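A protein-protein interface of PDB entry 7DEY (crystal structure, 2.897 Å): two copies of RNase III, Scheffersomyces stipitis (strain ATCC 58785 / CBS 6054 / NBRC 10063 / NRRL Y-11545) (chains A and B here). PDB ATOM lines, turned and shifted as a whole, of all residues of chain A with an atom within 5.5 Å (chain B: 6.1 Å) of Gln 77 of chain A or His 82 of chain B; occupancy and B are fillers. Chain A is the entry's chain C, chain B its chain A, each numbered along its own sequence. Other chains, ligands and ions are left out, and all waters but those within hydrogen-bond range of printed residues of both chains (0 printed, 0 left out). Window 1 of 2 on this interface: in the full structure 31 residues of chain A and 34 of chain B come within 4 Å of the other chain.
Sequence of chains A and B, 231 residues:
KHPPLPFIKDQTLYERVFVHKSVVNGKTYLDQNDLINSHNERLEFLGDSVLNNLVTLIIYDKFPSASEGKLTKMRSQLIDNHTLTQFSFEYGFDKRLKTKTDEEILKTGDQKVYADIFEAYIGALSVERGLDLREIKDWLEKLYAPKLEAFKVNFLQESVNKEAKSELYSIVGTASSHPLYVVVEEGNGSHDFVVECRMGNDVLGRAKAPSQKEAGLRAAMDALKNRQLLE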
ATOM      1  N   THR A  72      23.634  12.974  -9.084  1.00  0.00           N
ATOM      2  CA  THR A  72      22.465  12.898  -9.947  1.00  0.00           C
ATOM      3  C   THR A  72      22.707  13.651 -11.252  1.00  0.00           C
ATOM      4  O   THR A  72      22.338  13.169 -12.329  1.00  0.00           O
ATOM      5  CB  THR A  72      21.231  13.414  -9.199  1.00  0.00           C
ATOM      6  OG1 THR A  72      20.914  12.509  -8.132  1.00  0.00           O
ATOM      7  CG2 THR A  72      20.042  13.532 -10.114  1.00  0.00           C
ATOM      8  N   LYS A  73      23.402  14.791 -11.189  1.00  0.00           N
ATOM      9  CA  LYS A  73      23.651  15.561 -12.407  1.00  0.00           C
ATOM     10  C   LYS A  73      24.685  14.876 -13.293  1.00  0.00           C
ATOM     11  O   LYS A  73      24.494  14.785 -14.516  1.00  0.00           O
ATOM     12  CB  LYS A  73      24.083  16.992 -12.051  1.00  0.00           C
ATOM     13  CG  LYS A  73      22.935  17.878 -11.519  1.00  0.00           C
ATOM     14  CD  LYS A  73      23.371  19.272 -11.131  1.00  0.00           C
ATOM     15  CE  LYS A  73      22.293  19.993 -10.311  1.00  0.00           C
ATOM     16  NZ  LYS A  73      22.110  19.425  -8.933  1.00  0.00           N
ATOM     17  N   MET A  74      25.771  14.370 -12.688  1.00  0.00           N
ATOM     18  CA  MET A  74      26.766  13.591 -13.425  1.00  0.00           C
ATOM     19  C   MET A  74      26.130  12.420 -14.153  1.00  0.00           C
ATOM     20  O   MET A  74      26.479  12.129 -15.308  1.00  0.00           O
ATOM     21  CB  MET A  74      27.833  13.058 -12.477  1.00  0.00           C
ATOM     22  CG  MET A  74      29.037  13.936 -12.316  1.00  0.00           C
ATOM     23  SD  MET A  74      29.973  13.430 -10.855  1.00  0.00           S
ATOM     24  CE  MET A  74      31.625  13.913 -11.331  1.00  0.00           C
ATOM     25  N   ARG A  75      25.212  11.715 -13.480  1.00  0.00           N
ATOM     26  CA  ARG A  75      24.643  10.529 -14.099  1.00  0.00           C
ATOM     27  C   ARG A  75      23.746  10.900 -15.268  1.00  0.00           C
ATOM     28  O   ARG A  75      23.849  10.295 -16.348  1.00  0.00           O
ATOM     29  CB  ARG A  75      23.884   9.684 -13.077  1.00  0.00           C
ATOM     30  CG  ARG A  75      23.428   8.367 -13.690  1.00  0.00           C
ATOM     31  CD  ARG A  75      22.450   7.605 -12.819  1.00  0.00           C
ATOM     32  NE  ARG A  75      21.534   8.490 -12.130  1.00  0.00           N
ATOM     33  CZ  ARG A  75      20.876   8.173 -11.025  1.00  0.00           C
ATOM     34  NH1 ARG A  75      21.032   6.977 -10.461  1.00  0.00           N
ATOM     35  NH2 ARG A  75      20.057   9.066 -10.486  1.00  0.00           N
ATOM     36  N   SER A  76      22.890  11.913 -15.089  1.00  0.00           N
ATOM     37  CA  SER A  76      22.038  12.319 -16.194  1.00  0.00           C
ATOM     38  C   SER A  76      22.867  12.774 -17.390  1.00  0.00           C
ATOM     39  O   SER A  76      22.463  12.572 -18.544  1.00  0.00           O
ATOM     40  CB  SER A  76      21.079  13.403 -15.725  1.00  0.00           C
ATOM     41  OG  SER A  76      21.576  14.685 -16.022  1.00  0.00           O
ATOM     42  N   GLN A  77      24.057  13.330 -17.138  1.00  0.00           N
ATOM     43  CA  GLN A  77      24.915  13.778 -18.222  1.00  0.00           C
ATOM     44  C   GLN A  77      25.557  12.618 -18.977  1.00  0.00           C
ATOM     45  O   GLN A  77      25.716  12.714 -20.196  1.00  0.00           O
ATOM     46  CB  GLN A  77      25.968  14.725 -17.669  1.00  0.00           C
ATOM     47  CG  GLN A  77      25.401  16.086 -17.265  1.00  0.00           C
ATOM     48  CD  GLN A  77      24.932  16.920 -18.450  1.00  0.00           C
ATOM     49  OE1 GLN A  77      25.749  17.491 -19.177  1.00  0.00           O
ATOM     50  NE2 GLN A  77      23.613  16.988 -18.651  1.00  0.00           N
ATOM     51  N   LEU A  78      25.906  11.505 -18.304  1.00  0.00           N
ATOM     52  CA  LEU A  78      26.530  10.388 -19.014  1.00  0.00           C
ATOM     53  C   LEU A  78      25.549   9.348 -19.561  1.00  0.00           C
ATOM     54  O   LEU A  78      25.946   8.568 -20.435  1.00  0.00           O
ATOM     55  CB  LEU A  78      27.550   9.678 -18.130  1.00  0.00           C
ATOM     56  CG  LEU A  78      28.408  10.566 -17.215  1.00  0.00           C
ATOM     57  CD1 LEU A  78      28.960   9.749 -16.057  1.00  0.00           C
ATOM     58  CD2 LEU A  78      29.546  11.269 -17.946  1.00  0.00           C
ATOM     59  N   ILE A  79      24.292   9.292 -19.101  1.00  0.00           N
ATOM     60  CA  ILE A  79      23.326   8.382 -19.721  1.00  0.00           C
ATOM     61  C   ILE A  79      22.501   9.048 -20.807  1.00  0.00           C
ATOM     62  O   ILE A  79      21.564   8.410 -21.323  1.00  0.00           O
ATOM     63  CB  ILE A  79      22.331   7.735 -18.724  1.00  0.00           C
ATOM     64  CG1 ILE A  79      21.654   8.780 -17.837  1.00  0.00           C
ATOM     65  CG2 ILE A  79      22.945   6.576 -17.936  1.00  0.00           C
ATOM     66  CD1 ILE A  79      20.275   9.187 -18.290  1.00  0.00           C
ATOM     67  N   ASP A  80      22.770  10.309 -21.159  1.00  0.00           N
ATOM     68  CA  ASP A  80      21.800  10.948 -22.038  1.00  0.00           C
ATOM     69  C   ASP A  80      22.141  10.755 -23.523  1.00  0.00           C
ATOM     70  O   ASP A  80      23.160  10.171 -23.897  1.00  0.00           O
ATOM     71  CB  ASP A  80      21.620  12.414 -21.665  1.00  0.00           C
ATOM     72  CG  ASP A  80      22.875  13.193 -21.758  1.00  0.00           C
ATOM     73  OD1 ASP A  80      23.801  12.749 -22.477  1.00  0.00           O
ATOM     74  OD2 ASP A  80      22.926  14.276 -21.123  1.00  0.00           O
ATOM     75  N   HIS A  82      23.027  12.585 -26.077  1.00  0.00           N
ATOM     76  CA  HIS A  82      24.262  13.115 -26.649  1.00  0.00           C
ATOM     77  C   HIS A  82      25.420  12.132 -26.496  1.00  0.00           C
ATOM     78  O   HIS A  82      26.066  11.759 -27.480  1.00  0.00           O
ATOM     79  CB  HIS A  82      24.612  14.443 -25.984  1.00  0.00           C
ATOM     80  CG  HIS A  82      25.972  14.960 -26.335  1.00  0.00           C
ATOM     81  ND1 HIS A  82      27.121  14.542 -25.695  1.00  0.00           N
ATOM     82  CD2 HIS A  82      26.371  15.841 -27.283  1.00  0.00           C
ATOM     83  CE1 HIS A  82      28.165  15.159 -26.219  1.00  0.00           C
ATOM     84  NE2 HIS A  82      27.737  15.953 -27.185  1.00  0.00           N
ATOM     85  N   THR A  83      25.703  11.700 -25.267  1.00  0.00           N
ATOM     86  CA  THR A  83      26.869  10.847 -25.083  1.00  0.00           C
ATOM     87  C   THR A  83      26.652   9.434 -25.622  1.00  0.00           C
ATOM     88  O   THR A  83      27.598   8.822 -26.143  1.00  0.00           O
ATOM     89  CB  THR A  83      27.261  10.775 -23.625  1.00  0.00           C
ATOM     90  OG1 THR A  83      28.166   9.688 -23.478  1.00  0.00           O
ATOM     91  CG2 THR A  83      26.060  10.522 -22.778  1.00  0.00           C
ATOM     92  N   LYS A 147      35.602  10.926 -20.058  1.00  0.00           N
ATOM     93  CA  LYS A 147      34.498  11.732 -19.545  1.00  0.00           C
ATOM     94  C   LYS A 147      34.627  11.943 -18.047  1.00  0.00           C
ATOM     95  O   LYS A 147      34.252  13.007 -17.533  1.00  0.00           O
ATOM     96  CB  LYS A 147      33.143  11.081 -19.862  1.00  0.00           C
ATOM     97  CG  LYS A 147      32.993  10.611 -21.298  1.00  0.00           C
ATOM     98  CD  LYS A 147      31.653  10.998 -21.900  1.00  0.00           C
ATOM     99  CE  LYS A 147      31.634  12.414 -22.427  1.00  0.00           C
ATOM    100  NZ  LYS A 147      32.337  12.502 -23.724  1.00  0.00           N
ATOM    101  N   PHE A 151      35.327  15.337 -15.636  1.00  0.00           N
ATOM    102  CA  PHE A 151      34.554  15.811 -14.499  1.00  0.00           C
ATOM    103  C   PHE A 151      35.431  15.973 -13.261  1.00  0.00           C
ATOM    104  O   PHE A 151      35.197  16.877 -12.448  1.00  0.00           O
ATOM    105  CB  PHE A 151      33.389  14.868 -14.215  1.00  0.00           C
ATOM    106  CG  PHE A 151      32.308  14.890 -15.267  1.00  0.00           C
ATOM    107  CD1 PHE A 151      32.558  15.361 -16.559  1.00  0.00           C
ATOM    108  CD2 PHE A 151      31.038  14.419 -14.973  1.00  0.00           C
ATOM    109  CE1 PHE A 151      31.568  15.369 -17.530  1.00  0.00           C
ATOM    110  CE2 PHE A 151      30.038  14.427 -15.938  1.00  0.00           C
ATOM    111  CZ  PHE A 151      30.307  14.902 -17.217  1.00  0.00           C
ATOM    112  N   ILE B  79      27.589  22.941 -29.340  1.00  0.00           N
ATOM    113  CA  ILE B  79      26.553  23.920 -29.042  1.00  0.00           C
ATOM    114  C   ILE B  79      25.274  23.272 -28.566  1.00  0.00           C
ATOM    115  O   ILE B  79      24.354  23.988 -28.133  1.00  0.00           O
ATOM    116  CB  ILE B  79      26.273  24.828 -30.263  1.00  0.00           C
ATOM    117  CG1 ILE B  79      27.569  25.486 -30.726  1.00  0.00           C
ATOM    118  CG2 ILE B  79      25.310  25.946 -29.930  1.00  0.00           C
ATOM    119  CD1 ILE B  79      28.314  26.109 -29.582  1.00  0.00           C
ATOM    120  N   ASP B  80      25.178  21.952 -28.609  1.00  0.00           N
ATOM    121  CA  ASP B  80      23.926  21.323 -28.238  1.00  0.00           C
ATOM    122  C   ASP B  80      23.637  21.527 -26.760  1.00  0.00           C
ATOM    123  O   ASP B  80      24.482  21.991 -25.984  1.00  0.00           O
ATOM    124  CB  ASP B  80      23.962  19.842 -28.541  1.00  0.00           C
ATOM    125  CG  ASP B  80      25.156  19.169 -27.938  1.00  0.00           C
ATOM    126  OD1 ASP B  80      25.707  18.284 -28.618  1.00  0.00           O
ATOM    127  OD2 ASP B  80      25.567  19.527 -26.804  1.00  0.00           O
ATOM    128  N   ASN B  81      22.425  21.135 -26.369  1.00  0.00           N
ATOM    129  CA  ASN B  81      21.967  21.372 -25.006  1.00  0.00           C
ATOM    130  C   ASN B  81      22.818  20.617 -23.997  1.00  0.00           C
ATOM    131  O   ASN B  81      23.078  21.122 -22.895  1.00  0.00           O
ATOM    132  CB  ASN B  81      20.500  20.976 -24.899  1.00  0.00           C
ATOM    133  CG  ASN B  81      19.666  21.507 -26.063  1.00  0.00           C
ATOM    134  OD1 ASN B  81      19.774  21.022 -27.199  1.00  0.00           O
ATOM    135  ND2 ASN B  81      18.826  22.498 -25.784  1.00  0.00           N
ATOM    136  N   HIS B  82      23.303  19.437 -24.389  1.00  0.00           N
ATOM    137  CA  HIS B  82      24.094  18.593 -23.503  1.00  0.00           C
ATOM    138  C   HIS B  82      25.315  19.332 -22.965  1.00  0.00           C
ATOM    139  O   HIS B  82      25.477  19.491 -21.750  1.00  0.00           O
ATOM    140  CB  HIS B  82      24.515  17.334 -24.254  1.00  0.00           C
ATOM    141  CG  HIS B  82      25.394  16.425 -23.454  1.00  0.00           C
ATOM    142  ND1 HIS B  82      26.767  16.427 -23.560  1.00  0.00           N
ATOM    143  CD2 HIS B  82      25.093  15.500 -22.514  1.00  0.00           C
ATOM    144  CE1 HIS B  82      27.272  15.528 -22.733  1.00  0.00           C
ATOM    145  NE2 HIS B  82      26.276  14.952 -22.086  1.00  0.00           N
ATOM    146  N   THR B  83      26.203  19.785 -23.855  1.00  0.00           N
ATOM    147  CA  THR B  83      27.410  20.436 -23.368  1.00  0.00           C
ATOM    148  C   THR B  83      27.095  21.825 -22.827  1.00  0.00           C
ATOM    149  O   THR B  83      27.680  22.264 -21.831  1.00  0.00           O
ATOM    150  CB  THR B  83      28.453  20.484 -24.472  1.00  0.00           C
ATOM    151  OG1 THR B  83      28.100  21.489 -25.421  1.00  0.00           O
ATOM    152  CG2 THR B  83      28.465  19.155 -25.192  1.00  0.00           C
ATOM    153  N   LEU B  84      26.166  22.526 -23.464  1.00  0.00           N
ATOM    154  CA  LEU B  84      25.628  23.743 -22.874  1.00  0.00           C
ATOM    155  C   LEU B  84      25.228  23.517 -21.410  1.00  0.00           C
ATOM    156  O   LEU B  84      25.696  24.216 -20.501  1.00  0.00           O
ATOM    157  CB  LEU B  84      24.422  24.205 -23.702  1.00  0.00           C
ATOM    158  CG  LEU B  84      24.336  25.699 -23.892  1.00  0.00           C
ATOM    159  CD1 LEU B  84      25.738  26.174 -23.968  1.00  0.00           C
ATOM    160  CD2 LEU B  84      23.650  25.971 -25.178  1.00  0.00           C
ATOM    161  N   THR B  85      24.364  22.522 -21.170  1.00  0.00           N
ATOM    162  CA  THR B  85      23.852  22.258 -19.830  1.00  0.00           C
ATOM    163  C   THR B  85      24.970  21.885 -18.859  1.00  0.00           C
ATOM    164  O   THR B  85      24.830  22.097 -17.647  1.00  0.00           O
ATOM    165  CB  THR B  85      22.789  21.141 -19.889  1.00  0.00           C
ATOM    166  OG1 THR B  85      21.854  21.241 -18.805  1.00  0.00           O
ATOM    167  CG2 THR B  85      23.426  19.772 -19.872  1.00  0.00           C
ATOM    168  N   GLN B  86      26.075  21.316 -19.349  1.00  0.00           N
ATOM    169  CA  GLN B  86      27.096  20.939 -18.391  1.00  0.00           C
ATOM    170  C   GLN B  86      28.042  22.084 -18.090  1.00  0.00           C
ATOM    171  O   GLN B  86      28.648  22.104 -17.016  1.00  0.00           O
ATOM    172  CB  GLN B  86      27.887  19.743 -18.885  1.00  0.00           C
ATOM    173  CG  GLN B  86      28.782  20.081 -20.024  1.00  0.00           C
ATOM    174  CD  GLN B  86      30.140  19.475 -19.885  1.00  0.00           C
ATOM    175  OE1 GLN B  86      30.268  18.291 -19.571  1.00  0.00           O
ATOM    176  NE2 GLN B  86      31.178  20.283 -20.113  1.00  0.00           N
ATOM    177  N   PHE B  87      28.216  23.027 -19.019  1.00  0.00           N
ATOM    178  CA  PHE B  87      28.821  24.293 -18.638  1.00  0.00           C
ATOM    179  C   PHE B  87      27.957  24.979 -17.590  1.00  0.00           C
ATOM    180  O   PHE B  87      28.469  25.510 -16.592  1.00  0.00           O
ATOM    181  CB  PHE B  87      28.991  25.194 -19.860  1.00  0.00           C
ATOM    182  CG  PHE B  87      29.963  24.674 -20.892  1.00  0.00           C
ATOM    183  CD1 PHE B  87      30.922  23.738 -20.566  1.00  0.00           C
ATOM    184  CD2 PHE B  87      29.926  25.156 -22.185  1.00  0.00           C
ATOM    185  CE1 PHE B  87      31.815  23.286 -21.515  1.00  0.00           C
ATOM    186  CE2 PHE B  87      30.807  24.717 -23.132  1.00  0.00           C
ATOM    187  CZ  PHE B  87      31.758  23.780 -22.803  1.00  0.00           C
ATOM    188  N   PHE B  89      26.118  23.458 -15.471  1.00  0.00           N
ATOM    189  CA  PHE B  89      26.257  22.775 -14.191  1.00  0.00           C
ATOM    190  C   PHE B  89      27.627  22.981 -13.541  1.00  0.00           C
ATOM    191  O   PHE B  89      27.712  23.016 -12.313  1.00  0.00           O
ATOM    192  CB  PHE B  89      25.965  21.292 -14.365  1.00  0.00           C
ATOM    193  CG  PHE B  89      24.506  20.982 -14.419  1.00  0.00           C
ATOM    194  CD1 PHE B  89      23.588  21.874 -13.884  1.00  0.00           C
ATOM    195  CD2 PHE B  89      24.035  19.819 -15.037  1.00  0.00           C
ATOM    196  CE1 PHE B  89      22.214  21.605 -13.940  1.00  0.00           C
ATOM    197  CE2 PHE B  89      22.687  19.556 -15.086  1.00  0.00           C
ATOM    198  CZ  PHE B  89      21.772  20.449 -14.541  1.00  0.00           C
ATOM    199  N   ASP B 110      21.121  16.760 -21.222  1.00  0.00           N
ATOM    200  CA  ASP B 110      19.895  17.213 -21.863  1.00  0.00           C
ATOM    201  C   ASP B 110      19.450  18.533 -21.235  1.00  0.00           C
ATOM    202  O   ASP B 110      20.245  19.458 -21.133  1.00  0.00           O
ATOM    203  CB  ASP B 110      18.793  16.151 -21.743  1.00  0.00           C
ATOM    204  N   GLN B 111      18.184  18.626 -20.809  1.00  0.00           N
ATOM    205  CA  GLN B 111      17.688  19.870 -20.224  1.00  0.00           C
ATOM    206  C   GLN B 111      17.963  21.044 -21.152  1.00  0.00           C
ATOM    207  O   GLN B 111      18.947  21.764 -20.980  1.00  0.00           O
ATOM    208  CB  GLN B 111      18.272  20.112 -18.834  1.00  0.00           C
ATOM    209  CG  GLN B 111      18.241  18.879 -17.916  1.00  0.00           C
ATOM    210  CD  GLN B 111      16.840  18.322 -17.682  1.00  0.00           C
ATOM    211  OE1 GLN B 111      15.830  18.976 -17.970  1.00  0.00           O
ATOM    212  NE2 GLN B 111      16.778  17.107 -17.143  1.00  0.00           N
ATOM    213  N   ALA B 115      20.509  24.923 -20.912  1.00  0.00           N
ATOM    214  CA  ALA B 115      21.146  25.412 -22.126  1.00  0.00           C
ATOM    215  C   ALA B 115      20.711  26.834 -22.447  1.00  0.00           C
ATOM    216  O   ALA B 115      21.530  27.667 -22.863  1.00  0.00           O
ATOM    217  CB  ALA B 115      20.814  24.485 -23.292  1.00  0.00           C
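Of the 13 printed residues of chain B, 7 touch a printed residue of chain A. Hydrophobic or aromatic side chains of chain B within 4 Å of the printed part of chain A: His 82 and Phe 89. Along chain B the printed residues that touch a printed residue of chain A span positions 80 to 110.
Of the printed residues of chain B, Lys 73 of chain A touches Phe 89 (3.8 Å). Gln 77 of chain A touches four residues of chain B. Of the printed residues of chain A, Asp 80 of chain B touches His 82 (2.9 Å). Of chain A, only Gln 77 (3.0 Å), Asp 80 (2.9 Å) and His 82 (2.9 Å) come within 4 Å of His 82 of chain B. Of the printed residues of chain A, Thr 85 of chain B touches Gln 77 (3.0 Å). The nearest printed residue of chain A that does not touch Phe 89 of chain B is Gln 77 of chain A (4.5 Å).
The backbone NH of His 82 of chain B lies close to the side-chain carboxylate of Asp 80 of chain B (3.3 Å). The backbone carbonyl oxygen of Asp 110 of chain B sits close to the side-chain hydroxyl of Thr 85 of chain B, at 3.3 Å. OD2 of Asp 80 of chain B is in hydrogen-bond range of N of Thr 83 of chain B, at 3.0 Å. OG of Ser 76 of chain A lies within hydrogen-bond range of O of Lys 73 of chain A, at 3.3 Å.
A ring nitrogen (NE2) of His 82 of chain B sits close to the side-chain carboxylate of Asp 80 of chain A (3.3 Å). The side-chain carboxylate of Asp 80 of chain B sits close to a ring nitrogen (NE2) of His 82 of chain A. The backbone NH (N) of Asp 110 of chain B lies within hydrogen-bond range of the side-chain carboxylate (OD2) of Asp 80 of chain A. A ring nitrogen (ND1) of His 82 of chain B is in hydrogen-bond range of a ring nitrogen (ND1) of His 82 of chain A (2.9 Å). A ring nitrogen (NE2) of His 82 of chain B is in hydrogen-bond range of the backbone carbonyl oxygen (O) of Gln 77 of chain A (3.0 Å).
Asp 80 of chain A touches His 82 of chain B, and with the chains exchanged His 82 of chain A touches Asp 80 of chain B. His 82 of chain B touches its own counterpart, His 82 of chain A. His 82 of chain A touches Thr 83 of chain B, but with the chains exchanged Thr 83 of chain A does not touch His 82 of chain B (4.5 Å). Of the 11 pairs that touch across the chains among the printed residues, 3 have their exchanged pair printed and touching as well.
Among the printed residues, merely in contact across the chains: Lys 73 of chain A with Phe 89 of chain B, Gln 77 of chain A with Thr 85 of chain B, Gln 77 of chain A with Gln 86 of chain B, Gln 77 of chain A with Asp 110 of chain B, His 82 of chain A with Thr 83 of chain B and Phe 151 of chain A with Gln 86 of chain B.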
